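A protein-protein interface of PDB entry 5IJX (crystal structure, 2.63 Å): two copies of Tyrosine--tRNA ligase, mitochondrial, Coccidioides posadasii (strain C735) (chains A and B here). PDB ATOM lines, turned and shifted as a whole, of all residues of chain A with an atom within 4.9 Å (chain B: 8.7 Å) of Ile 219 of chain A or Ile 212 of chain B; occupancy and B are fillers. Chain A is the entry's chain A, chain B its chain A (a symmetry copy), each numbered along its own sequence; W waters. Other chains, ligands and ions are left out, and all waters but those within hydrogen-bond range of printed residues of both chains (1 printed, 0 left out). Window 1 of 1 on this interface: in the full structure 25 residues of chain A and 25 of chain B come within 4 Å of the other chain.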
ATOM      1  N   VAL A 181       4.011  31.125 -30.853  1.00  0.00           N
ATOM      2  CA  VAL A 181       4.682  31.710 -29.694  1.00  0.00           C
ATOM      3  C   VAL A 181       6.153  31.318 -29.683  1.00  0.00           C
ATOM      4  O   VAL A 181       7.037  32.160 -29.487  1.00  0.00           O
ATOM      5  CB  VAL A 181       3.976  31.290 -28.392  1.00  0.00           C
ATOM      6  CG1 VAL A 181       4.700  31.867 -27.192  1.00  0.00           C
ATOM      7  CG2 VAL A 181       2.523  31.752 -28.404  1.00  0.00           C
ATOM      8  N   MET A 182       6.437  30.037 -29.894  1.00  0.00           N
ATOM      9  CA  MET A 182       7.812  29.550 -29.871  1.00  0.00           C
ATOM     10  C   MET A 182       8.654  30.186 -30.974  1.00  0.00           C
ATOM     11  O   MET A 182       9.769  30.645 -30.727  1.00  0.00           O
ATOM     12  CB  MET A 182       7.839  28.027 -30.011  1.00  0.00           C
ATOM     13  CG  MET A 182       7.365  27.266 -28.780  1.00  0.00           C
ATOM     14  SD  MET A 182       8.450  27.639 -27.198  1.00  0.00           S
ATOM     15  CE  MET A 182       7.390  29.091 -26.429  1.00  0.00           C
ATOM     16  N   LEU A 185       8.509  34.376 -30.476  1.00  0.00           N
ATOM     17  CA  LEU A 185       9.051  34.828 -29.197  1.00  0.00           C
ATOM     18  C   LEU A 185      10.016  33.845 -28.555  1.00  0.00           C
ATOM     19  O   LEU A 185      11.041  34.264 -28.013  1.00  0.00           O
ATOM     20  CB  LEU A 185       7.908  35.112 -28.214  1.00  0.00           C
ATOM     21  CG  LEU A 185       8.322  35.595 -26.822  1.00  0.00           C
ATOM     22  CD1 LEU A 185       9.154  36.866 -26.902  1.00  0.00           C
ATOM     23  CD2 LEU A 185       7.094  35.821 -25.965  1.00  0.00           C
ATOM     24  N   GLY A 186       9.714  32.547 -28.596  1.00  0.00           N
ATOM     25  CA  GLY A 186      10.576  31.574 -27.940  1.00  0.00           C
ATOM     26  C   GLY A 186      12.013  31.634 -28.423  1.00  0.00           C
ATOM     27  O   GLY A 186      12.948  31.472 -27.636  1.00  0.00           O
ATOM     28  N   LEU A 189      13.791  34.777 -26.627  1.00  0.00           N
ATOM     29  CA  LEU A 189      14.063  34.671 -25.202  1.00  0.00           C
ATOM     30  C   LEU A 189      15.258  33.759 -24.956  1.00  0.00           C
ATOM     31  O   LEU A 189      15.426  32.735 -25.622  1.00  0.00           O
ATOM     32  CB  LEU A 189      12.833  34.134 -24.475  1.00  0.00           C
ATOM     33  CG  LEU A 189      11.569  34.972 -24.649  1.00  0.00           C
ATOM     34  CD1 LEU A 189      10.373  34.263 -24.036  1.00  0.00           C
ATOM     35  CD2 LEU A 189      11.759  36.344 -24.028  1.00  0.00           C
ATOM     36  N   ARG A 190      16.093  34.141 -23.993  1.00  0.00           N
ATOM     37  CA  ARG A 190      17.244  33.348 -23.586  1.00  0.00           C
ATOM     38  C   ARG A 190      16.984  32.744 -22.213  1.00  0.00           C
ATOM     39  O   ARG A 190      16.419  33.399 -21.332  1.00  0.00           O
ATOM     40  CB  ARG A 190      18.517  34.195 -23.554  1.00  0.00           C
ATOM     41  CG  ARG A 190      18.781  34.972 -24.839  1.00  0.00           C
ATOM     42  CD  ARG A 190      18.909  34.057 -26.051  1.00  0.00           C
ATOM     43  NE  ARG A 190      20.018  33.116 -25.917  1.00  0.00           N
ATOM     44  CZ  ARG A 190      20.348  32.210 -26.834  1.00  0.00           C
ATOM     45  NH1 ARG A 190      19.654  32.110 -27.962  1.00  0.00           N
ATOM     46  NH2 ARG A 190      21.374  31.397 -26.623  1.00  0.00           N
ATOM     47  N   LEU A 191      17.408  31.493 -22.035  1.00  0.00           N
ATOM     48  CA  LEU A 191      17.071  30.760 -20.820  1.00  0.00           C
ATOM     49  C   LEU A 191      17.771  31.350 -19.599  1.00  0.00           C
ATOM     50  O   LEU A 191      17.132  31.601 -18.570  1.00  0.00           O
ATOM     51  CB  LEU A 191      17.435  29.283 -20.989  1.00  0.00           C
ATOM     52  CG  LEU A 191      17.185  28.377 -19.784  1.00  0.00           C
ATOM     53  CD1 LEU A 191      15.697  28.277 -19.484  1.00  0.00           C
ATOM     54  CD2 LEU A 191      17.786  26.999 -20.024  1.00  0.00           C
ATOM     55  N   MET A 194      16.214  34.297 -17.756  1.00  0.00           N
ATOM     56  CA  MET A 194      14.981  33.916 -17.076  1.00  0.00           C
ATOM     57  C   MET A 194      15.264  33.125 -15.805  1.00  0.00           C
ATOM     58  O   MET A 194      14.637  33.358 -14.770  1.00  0.00           O
ATOM     59  CB  MET A 194      14.092  33.099 -18.005  1.00  0.00           C
ATOM     60  CG  MET A 194      13.458  33.922 -19.097  1.00  0.00           C
ATOM     61  SD  MET A 194      12.046  32.932 -19.975  1.00  0.00           S
ATOM     62  CE  MET A 194      10.657  33.070 -18.611  1.00  0.00           C
ATOM     63  N   PHE A 215       6.828  28.420 -14.723  1.00  0.00           N
ATOM     64  CA  PHE A 215       8.014  29.056 -15.288  1.00  0.00           C
ATOM     65  C   PHE A 215       7.675  29.877 -16.524  1.00  0.00           C
ATOM     66  O   PHE A 215       8.325  30.895 -16.789  1.00  0.00           O
ATOM     67  CB  PHE A 215       9.055  27.986 -15.616  1.00  0.00           C
ATOM     68  CG  PHE A 215      10.316  28.525 -16.224  1.00  0.00           C
ATOM     69  CD1 PHE A 215      11.208  29.262 -15.467  1.00  0.00           C
ATOM     70  CD2 PHE A 215      10.620  28.276 -17.551  1.00  0.00           C
ATOM     71  CE1 PHE A 215      12.374  29.752 -16.025  1.00  0.00           C
ATOM     72  CE2 PHE A 215      11.782  28.762 -18.114  1.00  0.00           C
ATOM     73  CZ  PHE A 215      12.660  29.503 -17.350  1.00  0.00           C
ATOM     74  N   CYS A 216       6.664  29.461 -17.283  1.00  0.00           N
ATOM     75  CA  CYS A 216       6.281  30.133 -18.517  1.00  0.00           C
ATOM     76  C   CYS A 216       5.238  31.225 -18.310  1.00  0.00           C
ATOM     77  O   CYS A 216       4.802  31.838 -19.290  1.00  0.00           O
ATOM     78  CB  CYS A 216       5.751  29.103 -19.524  1.00  0.00           C
ATOM     79  SG  CYS A 216       6.990  27.903 -20.071  1.00  0.00           S
ATOM     80  N   TYR A 217       4.830  31.487 -17.069  1.00  0.00           N
ATOM     81  CA  TYR A 217       3.858  32.549 -16.822  1.00  0.00           C
ATOM     82  C   TYR A 217       4.306  33.890 -17.387  1.00  0.00           C
ATOM     83  O   TYR A 217       3.538  34.505 -18.152  1.00  0.00           O
ATOM     84  CB  TYR A 217       3.581  32.648 -15.319  1.00  0.00           C
ATOM     85  CG  TYR A 217       2.499  33.642 -14.971  1.00  0.00           C
ATOM     86  CD1 TYR A 217       1.191  33.230 -14.764  1.00  0.00           C
ATOM     87  CD2 TYR A 217       2.786  34.997 -14.858  1.00  0.00           C
ATOM     88  CE1 TYR A 217       0.200  34.138 -14.448  1.00  0.00           C
ATOM     89  CE2 TYR A 217       1.802  35.912 -14.547  1.00  0.00           C
ATOM     90  CZ  TYR A 217       0.511  35.480 -14.341  1.00  0.00           C
ATOM     91  OH  TYR A 217      -0.469  36.394 -14.029  1.00  0.00           O
ATOM     92  N   PRO A 218       5.501  34.400 -17.075  1.00  0.00           N
ATOM     93  CA  PRO A 218       5.898  35.700 -17.639  1.00  0.00           C
ATOM     94  C   PRO A 218       5.941  35.700 -19.152  1.00  0.00           C
ATOM     95  O   PRO A 218       5.815  36.768 -19.763  1.00  0.00           O
ATOM     96  CB  PRO A 218       7.286  35.944 -17.030  1.00  0.00           C
ATOM     97  CG  PRO A 218       7.795  34.583 -16.686  1.00  0.00           C
ATOM     98  CD  PRO A 218       6.590  33.784 -16.294  1.00  0.00           C
ATOM     99  N   ILE A 219       6.112  34.540 -19.784  1.00  0.00           N
ATOM    100  CA  ILE A 219       6.021  34.484 -21.237  1.00  0.00           C
ATOM    101  C   ILE A 219       4.592  34.757 -21.680  1.00  0.00           C
ATOM    102  O   ILE A 219       4.351  35.549 -22.595  1.00  0.00           O
ATOM    103  CB  ILE A 219       6.520  33.127 -21.763  1.00  0.00           C
ATOM    104  CG1 ILE A 219       7.960  32.890 -21.311  1.00  0.00           C
ATOM    105  CG2 ILE A 219       6.415  33.096 -23.284  1.00  0.00           C
ATOM    106  CD1 ILE A 219       8.539  31.574 -21.759  1.00  0.00           C
ATOM    107  N   MET A 220       3.626  34.105 -21.046  1.00  0.00           N
ATOM    108  CA  MET A 220       2.234  34.316 -21.412  1.00  0.00           C
ATOM    109  C   MET A 220       1.861  35.776 -21.224  1.00  0.00           C
ATOM    110  O   MET A 220       1.210  36.374 -22.081  1.00  0.00           O
ATOM    111  CB  MET A 220       1.310  33.431 -20.585  1.00  0.00           C
ATOM    112  CG  MET A 220       1.494  31.947 -20.829  1.00  0.00           C
ATOM    113  SD  MET A 220       0.142  30.906 -19.899  1.00  0.00           S
ATOM    114  CE  MET A 220      -1.297  31.026 -21.206  1.00  0.00           C
ATOM    115  N   GLN A 221       2.281  36.359 -20.100  1.00  0.00           N
ATOM    116  CA  GLN A 221       1.957  37.761 -19.854  1.00  0.00           C
ATOM    117  C   GLN A 221       2.637  38.670 -20.873  1.00  0.00           C
ATOM    118  O   GLN A 221       2.023  39.620 -21.380  1.00  0.00           O
ATOM    119  CB  GLN A 221       2.352  38.141 -18.429  1.00  0.00           C
ATOM    120  CG  GLN A 221       2.187  39.613 -18.120  1.00  0.00           C
ATOM    121  CD  GLN A 221       2.151  39.894 -16.633  1.00  0.00           C
ATOM    122  OE1 GLN A 221       2.024  38.979 -15.817  1.00  0.00           O
ATOM    123  NE2 GLN A 221       2.263  41.166 -16.270  1.00  0.00           N
ATOM    124  N   GLY A 222       3.900  38.388 -21.194  1.00  0.00           N
ATOM    125  CA  GLY A 222       4.567  39.135 -22.243  1.00  0.00           C
ATOM    126  C   GLY A 222       3.860  39.020 -23.577  1.00  0.00           C
ATOM    127  O   GLY A 222       3.864  39.963 -24.370  1.00  0.00           O
ATOM    128  N   TRP A 223       3.241  37.869 -23.841  1.00  0.00           N
ATOM    129  CA  TRP A 223       2.524  37.677 -25.093  1.00  0.00           C
ATOM    130  C   TRP A 223       1.190  38.404 -25.086  1.00  0.00           C
ATOM    131  O   TRP A 223       0.729  38.847 -26.141  1.00  0.00           O
ATOM    132  CB  TRP A 223       2.308  36.186 -25.361  1.00  0.00           C
ATOM    133  CG  TRP A 223       1.821  35.912 -26.752  1.00  0.00           C
ATOM    134  CD1 TRP A 223       0.526  35.736 -27.152  1.00  0.00           C
ATOM    135  CD2 TRP A 223       2.625  35.795 -27.935  1.00  0.00           C
ATOM    136  NE1 TRP A 223       0.476  35.511 -28.510  1.00  0.00           N
ATOM    137  CE2 TRP A 223       1.751  35.545 -29.012  1.00  0.00           C
ATOM    138  CE3 TRP A 223       3.998  35.877 -28.185  1.00  0.00           C
ATOM    139  CZ2 TRP A 223       2.207  35.375 -30.318  1.00  0.00           C
ATOM    140  CZ3 TRP A 223       4.447  35.708 -29.480  1.00  0.00           C
ATOM    141  CH2 TRP A 223       3.555  35.458 -30.531  1.00  0.00           C
ATOM    142  N   PHE A 248      10.205  42.389 -18.338  1.00  0.00           N
ATOM    143  CA  PHE A 248      10.256  41.191 -19.172  1.00  0.00           C
ATOM    144  C   PHE A 248       9.385  41.340 -20.412  1.00  0.00           C
ATOM    145  O   PHE A 248       9.776  40.923 -21.509  1.00  0.00           O
ATOM    146  CB  PHE A 248       9.818  39.967 -18.365  1.00  0.00           C
ATOM    147  CG  PHE A 248       9.869  38.678 -19.139  1.00  0.00           C
ATOM    148  CD1 PHE A 248      10.935  37.809 -18.988  1.00  0.00           C
ATOM    149  CD2 PHE A 248       8.848  38.334 -20.015  1.00  0.00           C
ATOM    150  CE1 PHE A 248      10.987  36.620 -19.699  1.00  0.00           C
ATOM    151  CE2 PHE A 248       8.895  37.150 -20.729  1.00  0.00           C
ATOM    152  CZ  PHE A 248       9.965  36.292 -20.570  1.00  0.00           C
ATOM    153  N   ILE B 111      13.170  24.366 -34.997  1.00  0.00           N
ATOM    154  CA  ILE B 111      13.904  24.704 -33.786  1.00  0.00           C
ATOM    155  C   ILE B 111      15.223  23.948 -33.702  1.00  0.00           C
ATOM    156  O   ILE B 111      16.227  24.495 -33.243  1.00  0.00           O
ATOM    157  CB  ILE B 111      13.029  24.426 -32.545  1.00  0.00           C
ATOM    158  CG1 ILE B 111      11.766  25.292 -32.577  1.00  0.00           C
ATOM    159  CG2 ILE B 111      13.817  24.687 -31.270  1.00  0.00           C
ATOM    160  CD1 ILE B 111      10.732  24.892 -31.550  1.00  0.00           C
ATOM    161  N   PRO B 114      18.239  20.057 -29.620  1.00  0.00           N
ATOM    162  CA  PRO B 114      19.499  20.479 -28.988  1.00  0.00           C
ATOM    163  C   PRO B 114      20.360  19.337 -28.471  1.00  0.00           C
ATOM    164  O   PRO B 114      21.411  19.608 -27.880  1.00  0.00           O
ATOM    165  CB  PRO B 114      19.029  21.377 -27.835  1.00  0.00           C
ATOM    166  CG  PRO B 114      17.668  20.897 -27.517  1.00  0.00           C
ATOM    167  CD  PRO B 114      17.068  20.456 -28.819  1.00  0.00           C
ATOM    168  N   LEU B 178      -1.193  26.621 -27.170  1.00  0.00           N
ATOM    169  CA  LEU B 178      -0.272  26.657 -26.040  1.00  0.00           C
ATOM    170  C   LEU B 178      -1.008  26.370 -24.739  1.00  0.00           C
ATOM    171  O   LEU B 178      -0.475  25.701 -23.843  1.00  0.00           O
ATOM    172  CB  LEU B 178       0.424  28.018 -25.973  1.00  0.00           C
ATOM    173  CG  LEU B 178       1.334  28.279 -24.768  1.00  0.00           C
ATOM    174  CD1 LEU B 178       2.465  29.210 -25.168  1.00  0.00           C
ATOM    175  CD2 LEU B 178       0.560  28.877 -23.598  1.00  0.00           C
ATOM    176  N   MET B 182       0.179  23.675 -21.837  1.00  0.00           N
ATOM    177  CA  MET B 182       0.565  24.141 -20.509  1.00  0.00           C
ATOM    178  C   MET B 182      -0.292  23.505 -19.418  1.00  0.00           C
ATOM    179  O   MET B 182       0.228  23.026 -18.411  1.00  0.00           O
ATOM    180  CB  MET B 182       0.461  25.665 -20.429  1.00  0.00           C
ATOM    181  CG  MET B 182       1.538  26.418 -21.197  1.00  0.00           C
ATOM    182  SD  MET B 182       3.341  26.010 -20.564  1.00  0.00           S
ATOM    183  CE  MET B 182       3.786  24.566 -21.804  1.00  0.00           C
ATOM    184  N   LEU B 191      10.589  21.958 -13.296  1.00  0.00           N
ATOM    185  CA  LEU B 191      11.686  22.682 -13.928  1.00  0.00           C
ATOM    186  C   LEU B 191      13.037  22.067 -13.576  1.00  0.00           C
ATOM    187  O   LEU B 191      13.861  21.813 -14.462  1.00  0.00           O
ATOM    188  CB  LEU B 191      11.639  24.154 -13.515  1.00  0.00           C
ATOM    189  CG  LEU B 191      12.752  25.050 -14.058  1.00  0.00           C
ATOM    190  CD1 LEU B 191      12.658  25.170 -15.572  1.00  0.00           C
ATOM    191  CD2 LEU B 191      12.697  26.421 -13.399  1.00  0.00           C
ATOM    192  N   MET B 194      14.368  19.122 -15.592  1.00  0.00           N
ATOM    193  CA  MET B 194      14.711  19.514 -16.954  1.00  0.00           C
ATOM    194  C   MET B 194      16.024  20.285 -17.002  1.00  0.00           C
ATOM    195  O   MET B 194      16.858  20.050 -17.877  1.00  0.00           O
ATOM    196  CB  MET B 194      13.597  20.356 -17.562  1.00  0.00           C
ATOM    197  CG  MET B 194      12.365  19.556 -17.901  1.00  0.00           C
ATOM    198  SD  MET B 194      11.167  20.577 -19.026  1.00  0.00           S
ATOM    199  CE  MET B 194      12.122  20.444 -20.722  1.00  0.00           C
ATOM    200  N   LEU B 195      16.204  21.215 -16.063  1.00  0.00           N
ATOM    201  CA  LEU B 195      17.486  21.897 -15.944  1.00  0.00           C
ATOM    202  C   LEU B 195      18.616  20.939 -15.600  1.00  0.00           C
ATOM    203  O   LEU B 195      19.787  21.326 -15.702  1.00  0.00           O
ATOM    204  CB  LEU B 195      17.404  22.999 -14.886  1.00  0.00           C
ATOM    205  CG  LEU B 195      16.485  24.179 -15.205  1.00  0.00           C
ATOM    206  CD1 LEU B 195      16.542  25.204 -14.080  1.00  0.00           C
ATOM    207  CD2 LEU B 195      16.850  24.824 -16.541  1.00  0.00           C
ATOM    208  N   GLY B 209      24.502  29.223 -23.845  1.00  0.00           N
ATOM    209  CA  GLY B 209      23.108  29.349 -23.493  1.00  0.00           C
ATOM    210  C   GLY B 209      22.183  28.747 -24.531  1.00  0.00           C
ATOM    211  O   GLY B 209      22.590  28.059 -25.473  1.00  0.00           O
ATOM    212  N   MET B 210      20.898  29.024 -24.338  1.00  0.00           N
ATOM    213  CA  MET B 210      19.866  28.555 -25.246  1.00  0.00           C
ATOM    214  C   MET B 210      18.785  29.594 -25.422  1.00  0.00           C
ATOM    215  O   MET B 210      18.728  30.588 -24.700  1.00  0.00           O
ATOM    216  CB  MET B 210      19.206  27.277 -24.733  1.00  0.00           C
ATOM    217  CG  MET B 210      20.118  26.279 -24.073  1.00  0.00           C
ATOM    218  SD  MET B 210      19.031  24.917 -23.232  1.00  0.00           S
ATOM    219  CE  MET B 210      18.080  24.264 -24.795  1.00  0.00           C
ATOM    220  N   SER B 211      17.917  29.340 -26.389  1.00  0.00           N
ATOM    221  CA  SER B 211      16.630  30.004 -26.451  1.00  0.00           C
ATOM    222  C   SER B 211      15.605  29.188 -25.673  1.00  0.00           C
ATOM    223  O   SER B 211      15.814  28.010 -25.370  1.00  0.00           O
ATOM    224  CB  SER B 211      16.177  30.175 -27.901  1.00  0.00           C
ATOM    225  OG  SER B 211      15.871  28.923 -28.489  1.00  0.00           O
ATOM    226  N   ILE B 212      14.487  29.834 -25.338  1.00  0.00           N
ATOM    227  CA  ILE B 212      13.373  29.107 -24.739  1.00  0.00           C
ATOM    228  C   ILE B 212      12.832  28.074 -25.720  1.00  0.00           C
ATOM    229  O   ILE B 212      12.419  26.976 -25.327  1.00  0.00           O
ATOM    230  CB  ILE B 212      12.282  30.093 -24.282  1.00  0.00           C
ATOM    231  CG1 ILE B 212      12.812  30.980 -23.148  1.00  0.00           C
ATOM    232  CG2 ILE B 212      11.025  29.348 -23.857  1.00  0.00           C
ATOM    233  CD1 ILE B 212      13.298  30.218 -21.920  1.00  0.00           C
ATOM    234  N   ALA B 213      12.824  28.406 -27.012  1.00  0.00           N
ATOM    235  CA  ALA B 213      12.395  27.439 -28.016  1.00  0.00           C
ATOM    236  C   ALA B 213      13.235  26.168 -27.940  1.00  0.00           C
ATOM    237  O   ALA B 213      12.697  25.055 -27.914  1.00  0.00           O
ATOM    238  CB  ALA B 213      12.474  28.063 -29.408  1.00  0.00           C
ATOM    239  N   GLU B 214      14.562  26.315 -27.899  1.00  0.00           N
ATOM    240  CA  GLU B 214      15.430  25.149 -27.766  1.00  0.00           C
ATOM    241  C   GLU B 214      15.135  24.385 -26.481  1.00  0.00           C
ATOM    242  O   GLU B 214      15.066  23.149 -26.483  1.00  0.00           O
ATOM    243  CB  GLU B 214      16.896  25.578 -27.803  1.00  0.00           C
ATOM    244  CG  GLU B 214      17.367  26.116 -29.145  1.00  0.00           C
ATOM    245  CD  GLU B 214      18.801  26.606 -29.099  1.00  0.00           C
ATOM    246  OE1 GLU B 214      19.093  27.520 -28.299  1.00  0.00           O
ATOM    247  OE2 GLU B 214      19.638  26.068 -29.853  1.00  0.00           O
ATOM    248  N   PHE B 215      14.956  25.106 -25.373  1.00  0.00           N
ATOM    249  CA  PHE B 215      14.709  24.459 -24.089  1.00  0.00           C
ATOM    250  C   PHE B 215      13.414  23.658 -24.105  1.00  0.00           C
ATOM    251  O   PHE B 215      13.312  22.634 -23.421  1.00  0.00           O
ATOM    252  CB  PHE B 215      14.678  25.517 -22.986  1.00  0.00           C
ATOM    253  CG  PHE B 215      14.409  24.966 -21.616  1.00  0.00           C
ATOM    254  CD1 PHE B 215      15.359  24.206 -20.960  1.00  0.00           C
ATOM    255  CD2 PHE B 215      13.210  25.226 -20.976  1.00  0.00           C
ATOM    256  CE1 PHE B 215      15.115  23.705 -19.696  1.00  0.00           C
ATOM    257  CE2 PHE B 215      12.960  24.729 -19.713  1.00  0.00           C
ATOM    258  CZ  PHE B 215      13.914  23.965 -19.073  1.00  0.00           C
ATOM    259  N   CYS B 216      12.426  24.098 -24.880  1.00  0.00           N
ATOM    260  CA  CYS B 216      11.124  23.447 -24.938  1.00  0.00           C
ATOM    261  C   CYS B 216      11.037  22.369 -26.012  1.00  0.00           C
ATOM    262  O   CYS B 216       9.968  21.775 -26.186  1.00  0.00           O
ATOM    263  CB  CYS B 216      10.031  24.497 -25.177  1.00  0.00           C
ATOM    264  SG  CYS B 216       9.841  25.685 -23.824  1.00  0.00           S
ATOM    265  N   TYR B 217      12.126  22.099 -26.731  1.00  0.00           N
ATOM    266  CA  TYR B 217      12.097  21.049 -27.746  1.00  0.00           C
ATOM    267  C   TYR B 217      11.646  19.708 -27.182  1.00  0.00           C
ATOM    268  O   TYR B 217      10.699  19.114 -27.733  1.00  0.00           O
ATOM    269  CB  TYR B 217      13.475  20.937 -28.404  1.00  0.00           C
ATOM    270  CG  TYR B 217      13.515  19.955 -29.551  1.00  0.00           C
ATOM    271  CD1 TYR B 217      13.383  20.385 -30.863  1.00  0.00           C
ATOM    272  CD2 TYR B 217      13.678  18.594 -29.320  1.00  0.00           C
ATOM    273  CE1 TYR B 217      13.417  19.489 -31.913  1.00  0.00           C
ATOM    274  CE2 TYR B 217      13.709  17.692 -30.361  1.00  0.00           C
ATOM    275  CZ  TYR B 217      13.580  18.141 -31.656  1.00  0.00           C
ATOM    276  OH  TYR B 217      13.614  17.238 -32.694  1.00  0.00           O
ATOM    277  N   PRO B 218      12.250  19.176 -26.116  1.00  0.00           N
ATOM    278  CA  PRO B 218      11.787  17.877 -25.601  1.00  0.00           C
ATOM    279  C   PRO B 218      10.337  17.895 -25.168  1.00  0.00           C
ATOM    280  O   PRO B 218       9.698  16.835 -25.144  1.00  0.00           O
ATOM    281  CB  PRO B 218      12.732  17.605 -24.421  1.00  0.00           C
ATOM    282  CG  PRO B 218      13.217  18.953 -24.003  1.00  0.00           C
ATOM    283  CD  PRO B 218      13.295  19.766 -25.259  1.00  0.00           C
ATOM    284  N   ILE B 219       9.790  19.059 -24.825  1.00  0.00           N
ATOM    285  CA  ILE B 219       8.364  19.134 -24.535  1.00  0.00           C
ATOM    286  C   ILE B 219       7.561  18.888 -25.804  1.00  0.00           C
ATOM    287  O   ILE B 219       6.603  18.110 -25.809  1.00  0.00           O
ATOM    288  CB  ILE B 219       8.006  20.488 -23.901  1.00  0.00           C
ATOM    289  CG1 ILE B 219       8.818  20.698 -22.625  1.00  0.00           C
ATOM    290  CG2 ILE B 219       6.510  20.539 -23.608  1.00  0.00           C
ATOM    291  CD1 ILE B 219       8.557  22.010 -21.934  1.00  0.00           C
ATOM    292  N   MET B 220       7.933  19.547 -26.894  1.00  0.00           N
ATOM    293  CA  MET B 220       7.216  19.362 -28.146  1.00  0.00           C
ATOM    294  C   MET B 220       7.278  17.905 -28.572  1.00  0.00           C
ATOM    295  O   MET B 220       6.273  17.328 -28.986  1.00  0.00           O
ATOM    296  CB  MET B 220       7.789  20.251 -29.242  1.00  0.00           C
ATOM    297  CG  MET B 220       7.624  21.734 -28.983  1.00  0.00           C
ATOM    298  SD  MET B 220       8.188  22.785 -30.518  1.00  0.00           S
ATOM    299  CE  MET B 220       6.551  22.704 -31.570  1.00  0.00           C
HETATM  300  O   HOH W   1      20.849  29.621 -29.355  1.00  0.00           O
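Of the printed residues of chain B, Arg 190 of chain A touches Gly 209 (3.5 Å), Met 210 (3.1 Å) and Ser 211 (3.6 Å).
Of the printed residues of chain B, Leu 191 of chain A touches Met 210 (3.1 Å), Ile 212 (3.9 Å) and Phe 215 (3.8 Å).
No residue of chain B comes within 4 Å of Pro 218 of chain A.
Of chain B, only Ile 212 (3.9 Å) comes within 4 Å of Ile 219 of chain A.
Of the printed residues of chain A, Leu 178 of chain B touches Met 220 (3.7 Å).
Of the printed residues of chain A, Leu 191 of chain B touches Phe 215 (3.8 Å).
Leu 195 of chain B touches none of the printed residues of chain A.
Printed residues of chain A within 4 Å of Gly 209 of chain B: Arg 190.
Of chain A, only Gly 186 (3.2 Å), Leu 189 (3.1 Å), Leu 191 (3.9 Å), Met 194 (3.6 Å) and Ile 219 (3.9 Å) come within 4 Å of Ile 212 of chain B.
Ile 219 of chain B touches none of the printed residues of chain A.
The nearest printed residue of chain B that does not touch Met 194 of chain A is Leu 191 of chain B (7.3 Å).
Leu 191 of chain A touches Phe 215 of chain B, and with the chains exchanged Phe 215 of chain A touches Leu 191 of chain B.
9 positions are printed for both chains.
Of the 16 pairs that touch across the chains among the printed residues, 2 have their exchanged pair printed and touching as well.
Printed residues of chain A that touch a printed residue of chain B: Met 182, Gly 186, Leu 189, Arg 190, Leu 191, Met 194, Phe 215, Ile 219 and Met 220.
Of the 19 printed residues of chain B, 8 touch a printed residue of chain A.
Printed residues of chain B that touch a printed residue of chain A: Leu 178, Leu 191, Gly 209, Met 210, Ser 211, Ile 212, Ala 213 and Phe 215.
Hydrophobic or aromatic side chains of chain B within 4 Å of the printed part of chain A: Leu 178, Leu 191, Ile 212, Ala 213 and Phe 215.
Water W1 bridges OE1 of Glu 214 of chain B and NH1 of Arg 190 of chain A.
The backbone NH of Leu 191 of chain A is in hydrogen-bond range of the backbone carbonyl oxygen of Met 210 of chain B.
O of Gly 186 of chain A sits at hydrogen-bond distance from N of Ile 212 of chain B (3.2 Å).
The guanidinium group (NE) of Arg 190 of chain A lies within hydrogen-bond range of the backbone carbonyl oxygen (O) of Met 210 of chain B (3.1 Å).
The backbone NH (N) of Ile 212 of chain B sits at hydrogen-bond distance from the backbone carbonyl oxygen (O) of Leu 189 of chain A, 3.1 Å away.
The backbone NH (N) of Ala 213 of chain B sits at hydrogen-bond distance from the backbone carbonyl oxygen (O) of Gly 186 of chain A (3.1 Å).
O of Ile 212 of chain B lies within hydrogen-bond range of SG of Cys 216 of chain B (3.3 Å).
N of Ser 211 of chain B lies within hydrogen-bond range of OE1 of Glu 214 of chain B (2.9 Å).
The backbone carbonyl oxygen (O) of Val 181 of chain A lies within hydrogen-bond range of the backbone NH (N) of Gly 186 of chain A.
The side-chain hydroxyl (OG) of Ser 211 of chain B lies close to the backbone NH (N) of Ala 213 of chain B (3.4 Å).
Ala 213 of chain B touches Met 182 of chain A (CB to O, 3.97 Å).
Gly 186 of chain A touches Ser 211 of chain B.
O of Leu 189 of chain A touches CA of Ser 211 of chain B (3.1 Å).
Arg 190 of chain A touches Gly 209 of chain B (NH2 to C, 3.5 Å).
CD1 of Leu 191 of chain A touches CD1 of Ile 212 of chain B (3.9 Å).
CD2 of Leu 191 of chain A touches CD1 of Phe 215 of chain B (3.8 Å).
SD of Met 194 of chain A touches CD1 of Ile 212 of chain B, 3.6 Å away.
CD2 of Leu 191 of chain B touches CD1 of Phe 215 of chain A, at 3.8 Å.
Ile 219 of chain A touches Ile 212 of chain B.
Met 220 of chain A touches Leu 178 of chain B (CE to CD2, 3.7 Å).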
